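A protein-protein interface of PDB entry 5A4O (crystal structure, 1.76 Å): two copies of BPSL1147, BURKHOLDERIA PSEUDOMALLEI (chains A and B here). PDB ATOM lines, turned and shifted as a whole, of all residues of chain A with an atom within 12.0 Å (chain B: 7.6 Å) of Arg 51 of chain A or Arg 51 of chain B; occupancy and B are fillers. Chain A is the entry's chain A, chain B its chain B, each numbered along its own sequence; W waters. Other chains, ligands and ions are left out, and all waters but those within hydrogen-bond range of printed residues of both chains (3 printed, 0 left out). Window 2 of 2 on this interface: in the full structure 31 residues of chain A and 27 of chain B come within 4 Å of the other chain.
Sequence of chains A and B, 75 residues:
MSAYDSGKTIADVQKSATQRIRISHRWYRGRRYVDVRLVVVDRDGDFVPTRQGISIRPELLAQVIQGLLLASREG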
ATOM      1  N   ALA A   3      33.016   2.075  30.425  1.00  0.00           N
ATOM      2  CA  ALA A   3      31.805   1.267  30.277  1.00  0.00           C
ATOM      3  C   ALA A   3      31.934  -0.075  30.992  1.00  0.00           C
ATOM      4  O   ALA A   3      30.937  -0.798  31.134  1.00  0.00           O
ATOM      5  CB  ALA A   3      31.499   1.018  28.805  1.00  0.00           C
ATOM      6  N   LYS A  15      33.655  -5.601  17.667  1.00  0.00           N
ATOM      7  CA  LYS A  15      33.179  -5.262  16.313  1.00  0.00           C
ATOM      8  C   LYS A  15      34.287  -4.713  15.445  1.00  0.00           C
ATOM      9  O   LYS A  15      34.324  -4.959  14.228  1.00  0.00           O
ATOM     10  CB  LYS A  15      32.093  -4.190  16.364  1.00  0.00           C
ATOM     11  CG  LYS A  15      30.795  -4.678  16.940  1.00  0.00           C
ATOM     12  CD  LYS A  15      29.626  -3.684  16.789  1.00  0.00           C
ATOM     13  CE  LYS A  15      29.590  -2.977  15.442  1.00  0.00           C
ATOM     14  NZ  LYS A  15      28.200  -2.926  14.922  1.00  0.00           N
ATOM     15  N   GLN A  19      34.740  -0.303  18.505  1.00  0.00           N
ATOM     16  CA  GLN A  19      33.382  -0.616  18.944  1.00  0.00           C
ATOM     17  C   GLN A  19      33.340  -2.059  19.404  1.00  0.00           C
ATOM     18  O   GLN A  19      34.008  -2.930  18.823  1.00  0.00           O
ATOM     19  CB  GLN A  19      32.387  -0.466  17.794  1.00  0.00           C
ATOM     20  CG  GLN A  19      32.365   0.898  17.133  1.00  0.00           C
ATOM     21  CD  GLN A  19      31.080   1.165  16.388  1.00  0.00           C
ATOM     22  OE1 GLN A  19      30.476   0.278  15.783  1.00  0.00           O
ATOM     23  NE2 GLN A  19      30.644   2.419  16.432  1.00  0.00           N
ATOM     24  N   ARG A  20      32.571  -2.308  20.451  1.00  0.00           N
ATOM     25  CA  ARG A  20      32.355  -3.659  20.941  1.00  0.00           C
ATOM     26  C   ARG A  20      30.939  -3.754  21.366  1.00  0.00           C
ATOM     27  O   ARG A  20      30.292  -2.738  21.601  1.00  0.00           O
ATOM     28  CB  ARG A  20      33.248  -3.947  22.137  1.00  0.00           C
ATOM     29  CG  ARG A  20      34.706  -3.947  21.817  1.00  0.00           C
ATOM     30  CD  ARG A  20      35.515  -4.216  23.077  1.00  0.00           C
ATOM     31  NE  ARG A  20      36.926  -4.068  22.823  1.00  0.00           N
ATOM     32  CZ  ARG A  20      37.880  -4.181  23.743  1.00  0.00           C
ATOM     33  NH1 ARG A  20      37.590  -4.456  25.003  1.00  0.00           N
ATOM     34  NH2 ARG A  20      39.137  -4.000  23.388  1.00  0.00           N
ATOM     35  N   ILE A  21      30.442  -4.974  21.424  1.00  0.00           N
ATOM     36  CA  ILE A  21      29.154  -5.239  22.030  1.00  0.00           C
ATOM     37  C   ILE A  21      29.432  -5.860  23.405  1.00  0.00           C
ATOM     38  O   ILE A  21      29.978  -6.971  23.491  1.00  0.00           O
ATOM     39  CB  ILE A  21      28.286  -6.180  21.199  1.00  0.00           C
ATOM     40  CG1 ILE A  21      28.021  -5.615  19.798  1.00  0.00           C
ATOM     41  CG2 ILE A  21      26.999  -6.520  21.961  1.00  0.00           C
ATOM     42  CD1 ILE A  21      27.205  -4.343  19.754  1.00  0.00           C
ATOM     43  N   ARG A  22      29.065  -5.139  24.473  1.00  0.00           N
ATOM     44  CA  ARG A  22      29.292  -5.596  25.850  1.00  0.00           C
ATOM     45  C   ARG A  22      28.024  -6.203  26.442  1.00  0.00           C
ATOM     46  O   ARG A  22      26.954  -5.603  26.394  1.00  0.00           O
ATOM     47  CB  ARG A  22      29.770  -4.432  26.721  1.00  0.00           C
ATOM     48  CG  ARG A  22      30.040  -4.826  28.196  1.00  0.00           C
ATOM     49  CD  ARG A  22      30.541  -3.676  29.092  1.00  0.00           C
ATOM     50  NE  ARG A  22      30.733  -4.109  30.529  1.00  0.00           N
ATOM     51  CZ  ARG A  22      29.992  -3.749  31.604  1.00  0.00           C
ATOM     52  NH1 ARG A  22      28.976  -2.897  31.516  1.00  0.00           N
ATOM     53  NH2 ARG A  22      30.300  -4.221  32.812  1.00  0.00           N
ATOM     54  N   VAL A  34      19.996  -7.760  32.571  1.00  0.00           N
ATOM     55  CA  VAL A  34      20.988  -8.146  31.578  1.00  0.00           C
ATOM     56  C   VAL A  34      21.027  -7.040  30.528  1.00  0.00           C
ATOM     57  O   VAL A  34      19.997  -6.628  30.002  1.00  0.00           O
ATOM     58  CB  VAL A  34      20.674  -9.499  30.912  1.00  0.00           C
ATOM     59  CG1 VAL A  34      21.683  -9.817  29.805  1.00  0.00           C
ATOM     60  CG2 VAL A  34      20.686 -10.606  31.956  1.00  0.00           C
ATOM     61  N   ASP A  35      22.223  -6.554  30.237  1.00  0.00           N
ATOM     62  CA  ASP A  35      22.385  -5.450  29.326  1.00  0.00           C
ATOM     63  C   ASP A  35      23.212  -5.910  28.133  1.00  0.00           C
ATOM     64  O   ASP A  35      24.218  -6.619  28.297  1.00  0.00           O
ATOM     65  CB  ASP A  35      23.089  -4.340  30.091  1.00  0.00           C
ATOM     66  CG  ASP A  35      22.993  -3.012  29.424  1.00  0.00           C
ATOM     67  OD1 ASP A  35      21.941  -2.371  29.544  1.00  0.00           O
ATOM     68  OD2 ASP A  35      24.000  -2.580  28.822  1.00  0.00           O
ATOM     69  N   VAL A  36      22.798  -5.511  26.933  1.00  0.00           N
ATOM     70  CA  VAL A  36      23.513  -5.845  25.699  1.00  0.00           C
ATOM     71  C   VAL A  36      23.661  -4.532  24.973  1.00  0.00           C
ATOM     72  O   VAL A  36      22.664  -3.932  24.615  1.00  0.00           O
ATOM     73  CB  VAL A  36      22.716  -6.827  24.827  1.00  0.00           C
ATOM     74  CG1 VAL A  36      23.443  -7.117  23.538  1.00  0.00           C
ATOM     75  CG2 VAL A  36      22.425  -8.102  25.607  1.00  0.00           C
ATOM     76  N   ARG A  37      24.889  -4.053  24.795  1.00  0.00           N
ATOM     77  CA  ARG A  37      25.073  -2.608  24.473  1.00  0.00           C
ATOM     78  C   ARG A  37      26.305  -2.357  23.681  1.00  0.00           C
ATOM     79  O   ARG A  37      27.366  -2.865  24.016  1.00  0.00           O
ATOM     80  CB  ARG A  37      25.167  -1.792  25.777  1.00  0.00           C
ATOM     81  CG  ARG A  37      25.028  -0.262  25.626  1.00  0.00           C
ATOM     82  CD  ARG A  37      24.728   0.417  26.963  1.00  0.00           C
ATOM     83  NE  ARG A  37      23.460  -0.051  27.510  1.00  0.00           N
ATOM     84  CZ  ARG A  37      22.252   0.347  27.125  1.00  0.00           C
ATOM     85  NH1 ARG A  37      22.072   1.305  26.230  1.00  0.00           N
ATOM     86  NH2 ARG A  37      21.183  -0.200  27.696  1.00  0.00           N
ATOM     87  N   LEU A  38      26.147  -1.534  22.647  1.00  0.00           N
ATOM     88  CA  LEU A  38      27.248  -0.979  21.899  1.00  0.00           C
ATOM     89  C   LEU A  38      28.063  -0.010  22.791  1.00  0.00           C
ATOM     90  O   LEU A  38      27.527   0.969  23.352  1.00  0.00           O
ATOM     91  CB  LEU A  38      26.730  -0.281  20.641  1.00  0.00           C
ATOM     92  CG  LEU A  38      27.811   0.400  19.792  1.00  0.00           C
ATOM     93  CD1 LEU A  38      28.665  -0.671  19.191  1.00  0.00           C
ATOM     94  CD2 LEU A  38      27.214   1.316  18.721  1.00  0.00           C
ATOM     95  N   VAL A  39      29.349  -0.304  22.917  1.00  0.00           N
ATOM     96  CA  VAL A  39      30.298   0.539  23.624  1.00  0.00           C
ATOM     97  C   VAL A  39      31.359   0.994  22.623  1.00  0.00           C
ATOM     98  O   VAL A  39      31.679   0.256  21.704  1.00  0.00           O
ATOM     99  CB  VAL A  39      30.911  -0.173  24.842  1.00  0.00           C
ATOM    100  CG1 VAL A  39      29.807  -0.668  25.772  1.00  0.00           C
ATOM    101  CG2 VAL A  39      31.823  -1.333  24.421  1.00  0.00           C
ATOM    102  N   VAL A  40      31.818   2.225  22.756  1.00  0.00           N
ATOM    103  CA  VAL A  40      32.721   2.834  21.780  1.00  0.00           C
ATOM    104  C   VAL A  40      33.904   3.549  22.430  1.00  0.00           C
ATOM    105  O   VAL A  40      33.798   4.052  23.505  1.00  0.00           O
ATOM    106  CB  VAL A  40      32.019   3.855  20.842  1.00  0.00           C
ATOM    107  CG1 VAL A  40      30.834   3.267  20.123  1.00  0.00           C
ATOM    108  CG2 VAL A  40      31.628   5.062  21.611  1.00  0.00           C
ATOM    109  N   VAL A  41      35.026   3.567  21.731  1.00  0.00           N
ATOM    110  CA  VAL A  41      36.223   4.083  22.315  1.00  0.00           C
ATOM    111  C   VAL A  41      36.107   5.558  22.586  1.00  0.00           C
ATOM    112  O   VAL A  41      35.454   6.276  21.899  1.00  0.00           O
ATOM    113  CB  VAL A  41      37.455   3.960  21.424  1.00  0.00           C
ATOM    114  CG1 VAL A  41      38.289   2.735  21.669  1.00  0.00           C
ATOM    115  CG2 VAL A  41      37.161   4.250  19.993  1.00  0.00           C
ATOM    116  N   PHE A  47      36.283   2.432  26.736  1.00  0.00           N
ATOM    117  CA  PHE A  47      35.081   2.291  25.962  1.00  0.00           C
ATOM    118  C   PHE A  47      34.006   2.921  26.777  1.00  0.00           C
ATOM    119  O   PHE A  47      34.050   2.887  27.970  1.00  0.00           O
ATOM    120  CB  PHE A  47      34.777   0.861  25.643  1.00  0.00           C
ATOM    121  CG  PHE A  47      35.636   0.312  24.571  1.00  0.00           C
ATOM    122  CD1 PHE A  47      36.877  -0.142  24.874  1.00  0.00           C
ATOM    123  CD2 PHE A  47      35.219   0.277  23.275  1.00  0.00           C
ATOM    124  CE1 PHE A  47      37.689  -0.669  23.897  1.00  0.00           C
ATOM    125  CE2 PHE A  47      36.034  -0.228  22.292  1.00  0.00           C
ATOM    126  CZ  PHE A  47      37.276  -0.692  22.619  1.00  0.00           C
ATOM    127  N   VAL A  48      33.073   3.527  26.095  1.00  0.00           N
ATOM    128  CA  VAL A  48      31.991   4.206  26.743  1.00  0.00           C
ATOM    129  C   VAL A  48      30.648   3.742  26.199  1.00  0.00           C
ATOM    130  O   VAL A  48      30.556   3.433  25.069  1.00  0.00           O
ATOM    131  CB  VAL A  48      32.140   5.687  26.528  1.00  0.00           C
ATOM    132  CG1 VAL A  48      31.092   6.446  27.263  1.00  0.00           C
ATOM    133  CG2 VAL A  48      33.521   6.096  26.976  1.00  0.00           C
ATOM    134  N   PRO A  49      29.636   3.638  27.050  1.00  0.00           N
ATOM    135  CA  PRO A  49      28.390   3.046  26.562  1.00  0.00           C
ATOM    136  C   PRO A  49      27.625   4.025  25.692  1.00  0.00           C
ATOM    137  O   PRO A  49      27.855   5.260  25.766  1.00  0.00           O
ATOM    138  CB  PRO A  49      27.612   2.749  27.853  1.00  0.00           C
ATOM    139  CG  PRO A  49      28.078   3.817  28.804  1.00  0.00           C
ATOM    140  CD  PRO A  49      29.544   3.998  28.483  1.00  0.00           C
ATOM    141  N   THR A  50      26.739   3.487  24.858  1.00  0.00           N
ATOM    142  CA  THR A  50      25.858   4.272  24.033  1.00  0.00           C
ATOM    143  C   THR A  50      24.414   3.926  24.361  1.00  0.00           C
ATOM    144  O   THR A  50      24.180   3.056  25.153  1.00  0.00           O
ATOM    145  CB  THR A  50      26.069   3.962  22.557  1.00  0.00           C
ATOM    146  OG1 THR A  50      25.604   2.639  22.289  1.00  0.00           O
ATOM    147  CG2 THR A  50      27.554   4.040  22.175  1.00  0.00           C
ATOM    148  N   ARG A  51      23.465   4.568  23.681  1.00  0.00           N
ATOM    149  CA  ARG A  51      22.057   4.248  23.852  1.00  0.00           C
ATOM    150  C   ARG A  51      21.667   3.104  22.937  1.00  0.00           C
ATOM    151  O   ARG A  51      20.507   2.661  22.991  1.00  0.00           O
ATOM    152  CB  ARG A  51      21.177   5.455  23.548  1.00  0.00           C
ATOM    153  CG  ARG A  51      21.436   6.657  24.439  1.00  0.00           C
ATOM    154  CD  ARG A  51      20.418   7.783  24.195  1.00  0.00           C
ATOM    155  NE  ARG A  51      19.046   7.382  24.519  1.00  0.00           N
ATOM    156  CZ  ARG A  51      18.096   7.028  23.648  1.00  0.00           C
ATOM    157  NH1 ARG A  51      18.288   7.027  22.329  1.00  0.00           N
ATOM    158  NH2 ARG A  51      16.896   6.692  24.106  1.00  0.00           N
ATOM    159  N   GLN A  52      22.612   2.641  22.108  1.00  0.00           N
ATOM    160  CA  GLN A  52      22.361   1.508  21.199  1.00  0.00           C
ATOM    161  C   GLN A  52      22.504   0.208  21.964  1.00  0.00           C
ATOM    162  O   GLN A  52      23.542  -0.447  21.955  1.00  0.00           O
ATOM    163  CB  GLN A  52      23.235   1.575  19.955  1.00  0.00           C
ATOM    164  CG  GLN A  52      22.696   2.553  18.920  1.00  0.00           C
ATOM    165  CD  GLN A  52      22.588   3.981  19.419  1.00  0.00           C
ATOM    166  OE1 GLN A  52      23.577   4.685  19.509  1.00  0.00           O
ATOM    167  NE2 GLN A  52      21.372   4.423  19.735  1.00  0.00           N
ATOM    168  N   GLY A  53      21.474  -0.110  22.723  1.00  0.00           N
ATOM    169  CA  GLY A  53      21.504  -1.326  23.535  1.00  0.00           C
ATOM    170  C   GLY A  53      20.130  -1.691  24.014  1.00  0.00           C
ATOM    171  O   GLY A  53      19.151  -0.933  23.811  1.00  0.00           O
ATOM    172  N   ILE A  54      20.045  -2.858  24.623  1.00  0.00           N
ATOM    173  CA  ILE A  54      18.804  -3.261  25.250  1.00  0.00           C
ATOM    174  C   ILE A  54      19.066  -3.693  26.723  1.00  0.00           C
ATOM    175  O   ILE A  54      20.181  -4.134  27.104  1.00  0.00           O
ATOM    176  CB  ILE A  54      18.088  -4.366  24.434  1.00  0.00           C
ATOM    177  CG1 ILE A  54      18.937  -5.620  24.396  1.00  0.00           C
ATOM    178  CG2 ILE A  54      17.758  -3.907  23.020  1.00  0.00           C
ATOM    179  CD1 ILE A  54      18.196  -6.866  24.000  1.00  0.00           C
ATOM    180  N   SER A  55      18.009  -3.602  27.525  1.00  0.00           N
ATOM    181  CA  SER A  55      18.041  -3.963  28.936  1.00  0.00           C
ATOM    182  C   SER A  55      16.860  -4.858  29.171  1.00  0.00           C
ATOM    183  O   SER A  55      15.718  -4.439  28.917  1.00  0.00           O
ATOM    184  CB  SER A  55      17.908  -2.717  29.795  1.00  0.00           C
ATOM    185  OG  SER A  55      17.919  -3.064  31.151  1.00  0.00           O
ATOM    186  N   ILE A  56      17.123  -6.075  29.645  1.00  0.00           N
ATOM    187  CA  ILE A  56      16.063  -7.026  29.852  1.00  0.00           C
ATOM    188  C   ILE A  56      16.144  -7.772  31.165  1.00  0.00           C
ATOM    189  O   ILE A  56      17.208  -7.979  31.725  1.00  0.00           O
ATOM    190  CB  ILE A  56      16.042  -8.067  28.741  1.00  0.00           C
ATOM    191  CG1 ILE A  56      17.381  -8.792  28.652  1.00  0.00           C
ATOM    192  CG2 ILE A  56      15.716  -7.398  27.413  1.00  0.00           C
ATOM    193  CD1 ILE A  56      17.253 -10.087  27.947  1.00  0.00           C
ATOM    194  N   SER B   2      12.283   7.554  15.037  1.00  0.00           N
ATOM    195  CA  SER B   2      12.091   6.074  14.943  1.00  0.00           C
ATOM    196  C   SER B   2      12.934   5.495  13.817  1.00  0.00           C
ATOM    197  O   SER B   2      13.119   6.127  12.762  1.00  0.00           O
ATOM    198  CB  SER B   2      10.613   5.740  14.751  1.00  0.00           C
ATOM    199  OG  SER B   2       9.863   6.079  15.916  1.00  0.00           O
ATOM    200  N   ALA B   3      13.485   4.312  14.058  1.00  0.00           N
ATOM    201  CA  ALA B   3      14.421   3.723  13.115  1.00  0.00           C
ATOM    202  C   ALA B   3      13.691   3.356  11.810  1.00  0.00           C
ATOM    203  O   ALA B   3      12.469   3.114  11.775  1.00  0.00           O
ATOM    204  CB  ALA B   3      15.126   2.513  13.713  1.00  0.00           C
ATOM    205  N   VAL B  36      18.805  -6.234  16.721  1.00  0.00           N
ATOM    206  CA  VAL B  36      18.158  -6.540  17.970  1.00  0.00           C
ATOM    207  C   VAL B  36      17.813  -5.190  18.617  1.00  0.00           C
ATOM    208  O   VAL B  36      18.694  -4.415  18.923  1.00  0.00           O
ATOM    209  CB  VAL B  36      19.071  -7.353  18.923  1.00  0.00           C
ATOM    210  CG1 VAL B  36      18.320  -7.633  20.204  1.00  0.00           C
ATOM    211  CG2 VAL B  36      19.553  -8.639  18.239  1.00  0.00           C
ATOM    212  N   ARG B  37      16.519  -4.915  18.774  1.00  0.00           N
ATOM    213  CA  ARG B  37      16.036  -3.566  18.968  1.00  0.00           C
ATOM    214  C   ARG B  37      14.768  -3.484  19.781  1.00  0.00           C
ATOM    215  O   ARG B  37      13.858  -4.288  19.631  1.00  0.00           O
ATOM    216  CB  ARG B  37      15.807  -2.959  17.579  1.00  0.00           C
ATOM    217  CG  ARG B  37      15.507  -1.480  17.510  1.00  0.00           C
ATOM    218  CD  ARG B  37      15.562  -1.046  16.033  1.00  0.00           C
ATOM    219  NE  ARG B  37      16.901  -1.218  15.484  1.00  0.00           N
ATOM    220  CZ  ARG B  37      17.928  -0.390  15.694  1.00  0.00           C
ATOM    221  NH1 ARG B  37      17.789   0.759  16.372  1.00  0.00           N
ATOM    222  NH2 ARG B  37      19.105  -0.697  15.180  1.00  0.00           N
ATOM    223  N   LEU B  38      14.735  -2.498  20.663  1.00  0.00           N
ATOM    224  CA  LEU B  38      13.514  -2.148  21.326  1.00  0.00           C
ATOM    225  C   LEU B  38      12.526  -1.527  20.324  1.00  0.00           C
ATOM    226  O   LEU B  38      12.857  -0.538  19.624  1.00  0.00           O
ATOM    227  CB  LEU B  38      13.788  -1.224  22.496  1.00  0.00           C
ATOM    228  CG  LEU B  38      12.503  -0.742  23.177  1.00  0.00           C
ATOM    229  CD1 LEU B  38      11.750  -1.895  23.840  1.00  0.00           C
ATOM    230  CD2 LEU B  38      12.770   0.418  24.131  1.00  0.00           C
ATOM    231  N   VAL B  39      11.304  -2.079  20.296  1.00  0.00           N
ATOM    232  CA  VAL B  39      10.195  -1.554  19.503  1.00  0.00           C
ATOM    233  C   VAL B  39       9.003  -1.257  20.454  1.00  0.00           C
ATOM    234  O   VAL B  39       8.831  -1.970  21.460  1.00  0.00           O
ATOM    235  CB  VAL B  39       9.776  -2.487  18.315  1.00  0.00           C
ATOM    236  CG1 VAL B  39      10.998  -2.898  17.503  1.00  0.00           C
ATOM    237  CG2 VAL B  39       9.105  -3.753  18.770  1.00  0.00           C
ATOM    238  N   VAL B  48       6.668   0.040  16.526  1.00  0.00           N
ATOM    239  CA  VAL B  48       7.566   0.930  15.797  1.00  0.00           C
ATOM    240  C   VAL B  48       8.991   0.862  16.377  1.00  0.00           C
ATOM    241  O   VAL B  48       9.194   1.029  17.608  1.00  0.00           O
ATOM    242  CB  VAL B  48       7.032   2.378  15.907  1.00  0.00           C
ATOM    243  CG1 VAL B  48       8.013   3.370  15.304  1.00  0.00           C
ATOM    244  CG2 VAL B  48       5.667   2.495  15.235  1.00  0.00           C
ATOM    245  N   PRO B  49      10.013   0.686  15.503  1.00  0.00           N
ATOM    246  CA  PRO B  49      11.341   0.527  16.081  1.00  0.00           C
ATOM    247  C   PRO B  49      11.921   1.829  16.631  1.00  0.00           C
ATOM    248  O   PRO B  49      11.712   2.886  16.024  1.00  0.00           O
ATOM    249  CB  PRO B  49      12.195   0.015  14.911  1.00  0.00           C
ATOM    250  CG  PRO B  49      11.471   0.412  13.666  1.00  0.00           C
ATOM    251  CD  PRO B  49      10.022   0.650  14.024  1.00  0.00           C
ATOM    252  N   THR B  50      12.661   1.733  17.740  1.00  0.00           N
ATOM    253  CA  THR B  50      13.340   2.873  18.380  1.00  0.00           C
ATOM    254  C   THR B  50      14.813   2.859  17.993  1.00  0.00           C
ATOM    255  O   THR B  50      15.247   1.921  17.339  1.00  0.00           O
ATOM    256  CB  THR B  50      13.278   2.783  19.931  1.00  0.00           C
ATOM    257  OG1 THR B  50      14.115   1.717  20.384  1.00  0.00           O
ATOM    258  CG2 THR B  50      11.827   2.595  20.459  1.00  0.00           C
ATOM    259  N   ARG B  51      15.589   3.849  18.449  1.00  0.00           N
ATOM    260  CA  ARG B  51      17.041   3.835  18.275  1.00  0.00           C
ATOM    261  C   ARG B  51      17.779   2.906  19.255  1.00  0.00           C
ATOM    262  O   ARG B  51      18.993   2.711  19.137  1.00  0.00           O
ATOM    263  CB  ARG B  51      17.605   5.246  18.415  1.00  0.00           C
ATOM    264  CG  ARG B  51      17.209   6.161  17.274  1.00  0.00           C
ATOM    265  CD  ARG B  51      17.542   7.628  17.573  1.00  0.00           C
ATOM    266  NE  ARG B  51      16.995   8.045  18.858  1.00  0.00           N
ATOM    267  CZ  ARG B  51      17.437   9.070  19.596  1.00  0.00           C
ATOM    268  NH1 ARG B  51      18.432   9.861  19.176  1.00  0.00           N
ATOM    269  NH2 ARG B  51      16.851   9.330  20.767  1.00  0.00           N
ATOM    270  N   GLN B  52      17.073   2.336  20.214  1.00  0.00           N
ATOM    271  CA  GLN B  52      17.732   1.518  21.217  1.00  0.00           C
ATOM    272  C   GLN B  52      17.860   0.073  20.721  1.00  0.00           C
ATOM    273  O   GLN B  52      17.023  -0.804  20.990  1.00  0.00           O
ATOM    274  CB  GLN B  52      16.989   1.590  22.521  1.00  0.00           C
ATOM    275  CG  GLN B  52      16.835   3.011  23.072  1.00  0.00           C
ATOM    276  CD  GLN B  52      15.959   3.015  24.312  1.00  0.00           C
ATOM    277  OE1 GLN B  52      16.073   2.138  25.146  1.00  0.00           O
ATOM    278  NE2 GLN B  52      15.041   3.963  24.402  1.00  0.00           N
ATOM    279  N   GLY B  53      18.916  -0.160  19.982  1.00  0.00           N
ATOM    280  CA  GLY B  53      19.074  -1.423  19.279  1.00  0.00           C
ATOM    281  C   GLY B  53      20.478  -1.541  18.787  1.00  0.00           C
ATOM    282  O   GLY B  53      21.179  -0.534  18.696  1.00  0.00           O
ATOM    283  N   ILE B  54      20.889  -2.771  18.484  1.00  0.00           N
ATOM    284  CA  ILE B  54      22.224  -3.022  17.945  1.00  0.00           C
ATOM    285  C   ILE B  54      22.128  -3.844  16.666  1.00  0.00           C
ATOM    286  O   ILE B  54      21.213  -4.648  16.494  1.00  0.00           O
ATOM    287  CB  ILE B  54      23.142  -3.764  18.924  1.00  0.00           C
ATOM    288  CG1 ILE B  54      22.617  -5.175  19.219  1.00  0.00           C
ATOM    289  CG2 ILE B  54      23.288  -2.956  20.186  1.00  0.00           C
ATOM    290  CD1 ILE B  54      23.590  -6.061  19.975  1.00  0.00           C
HETATM  291  O   HOH W   1      19.526   2.494  25.526  1.00  0.00           O
HETATM  292  O   HOH W   2      18.377   0.301  26.707  1.00  0.00           O
HETATM  293  O   HOH W   3      16.674  -0.557  24.859  1.00  0.00           O
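Lys 15 of chain A touches none of the printed residues of chain B.
Of the printed residues of chain B, Ile 21 of chain A touches Ile 54.
Of the printed residues of chain B, Val 36 of chain A touches Ile 54.
Of chain B, only Arg 51 and Gln 52 come within 4 Å of Arg 51 of chain A.
Of the printed residues of chain B, Gly 53 of chain A touches Gln 52 and Gly 53.
No residue of chain A comes within 4 Å of Ser 2 of chain B.
Ala 3 of chain B touches none of the printed residues of chain A.
Arg 37 of chain B touches none of the printed residues of chain A.
No residue of chain A comes within 4 Å of Pro 49 of chain B.
No residue of chain A comes within 4 Å of Thr 50 of chain B.
Arg 51 of chain B touches two residues of chain A.
Gln 52 of chain B touches three residues of chain A.
Gly 53 of chain B touches just these residues of chain A: Gln 52 and Gly 53.
Of the printed residues of chain A, Ile 54 of chain B touches Ile 21, Val 36 and Gln 52.
The nearest residue of chain A that does not touch Arg 51 of chain B is Gly 53 of chain A (5.2 Å).
The nearest printed residue of chain A that does not touch Val 36 of chain B is Gly 53 of chain A (5.9 Å).
N of Leu 38 of chain B is in hydrogen-bond range of O of Gln 52 of chain B (2.9 Å).
The backbone NH (N) of Gln 52 of chain A is in hydrogen-bond range of the side-chain hydroxyl (OG1) of Thr 50 of chain A (3.0 Å).
N of Gln 52 of chain B lies within hydrogen-bond range of OG1 of Thr 50 of chain B, 3.0 Å away.
O of Val 36 of chain B sits at hydrogen-bond distance from N of Ile 54 of chain B (2.8 Å).
Val 36 of chain A touches Ile 54 of chain B, and with the chains exchanged Ile 54 of chain A touches Val 36 of chain B.
Arg 51 of chain A touches its own counterpart, Arg 51 of chain B.
Gln 52 of chain A touches Ile 54 of chain B, and with the chains exchanged Ile 54 of chain A touches Gln 52 of chain B.
12 positions are printed for both chains.
Of the 11 pairs that touch across the chains among the printed residues, 10 have their exchanged pair printed and touching as well.
Water W3 bridges O of Gly 53 of chain A and OE1 of Gln 52 of chain B.
Water W1 lies within hydrogen-bond range of the backbone carbonyl oxygen (O) of Arg 51 of chain A (2.7 Å), the guanidinium group (NH1) of Arg 37 of chain A (2.9 Å) and the side-chain amide oxygen (OE1) of Gln 52 of chain B (3.5 Å).
Water W2 lies within hydrogen-bond range of the guanidinium group (NH2) of Arg 37 of chain A (3.0 Å), the backbone carbonyl oxygen (O) of Gly 53 of chain A (3.2 Å) and the side-chain amide oxygen (OE1) of Gln 52 of chain B (3.3 Å).
NH1 of Arg 51 of chain A lies close to NH2 of Arg 51 of chain B.
The guanidinium group of Arg 51 of chain A sits close to the side-chain amide nitrogen of Gln 52 of chain B.
NE2 of Gln 52 of chain A is in hydrogen-bond range of O of Arg 51 of chain B (3.0 Å).
Of the 24 printed residues of chain A, 6 touch a printed residue of chain B.
Hydrophobic or aromatic side chains of chain A within 4 Å of the printed part of chain B: Ile 21, Val 36 and Ile 54.
Of the 13 printed residues of chain B, 5 touch a printed residue of chain A.
Printed residues of chain B that touch a printed residue of chain A: Val 36, Arg 51, Gln 52, Gly 53 and Ile 54.
Hydrophobic or aromatic side chains of chain B that line the printed part of chain A: Val 36 and Ile 54.
Along chain B the printed residues that touch a printed residue of chain A span positions 36 to 54.
Among the printed residues, no Asp or Glu carboxylate lies within 4 Å of a Lys or Arg side-chain nitrogen of the other chain.
Ile 54 of chain B touches Ile 21 of chain A (CD1 to CG2, 3.97 Å).
Val 36 of chain A touches Ile 54 of chain B.
CB of Gln 52 of chain A touches O of Gly 53 of chain B, 3.2 Å away.
CG2 of Ile 54 of chain B touches O of Gln 52 of chain A, 3.1 Å away.
Gly 53 of chain A touches Gln 52 of chain B.
N of Gly 53 of chain A touches N of Gly 53 of chain B, 3.7 Å away.
Ile 54 of chain A touches Val 36 of chain B.
Ile 54 of chain A touches Gln 52 of chain B.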
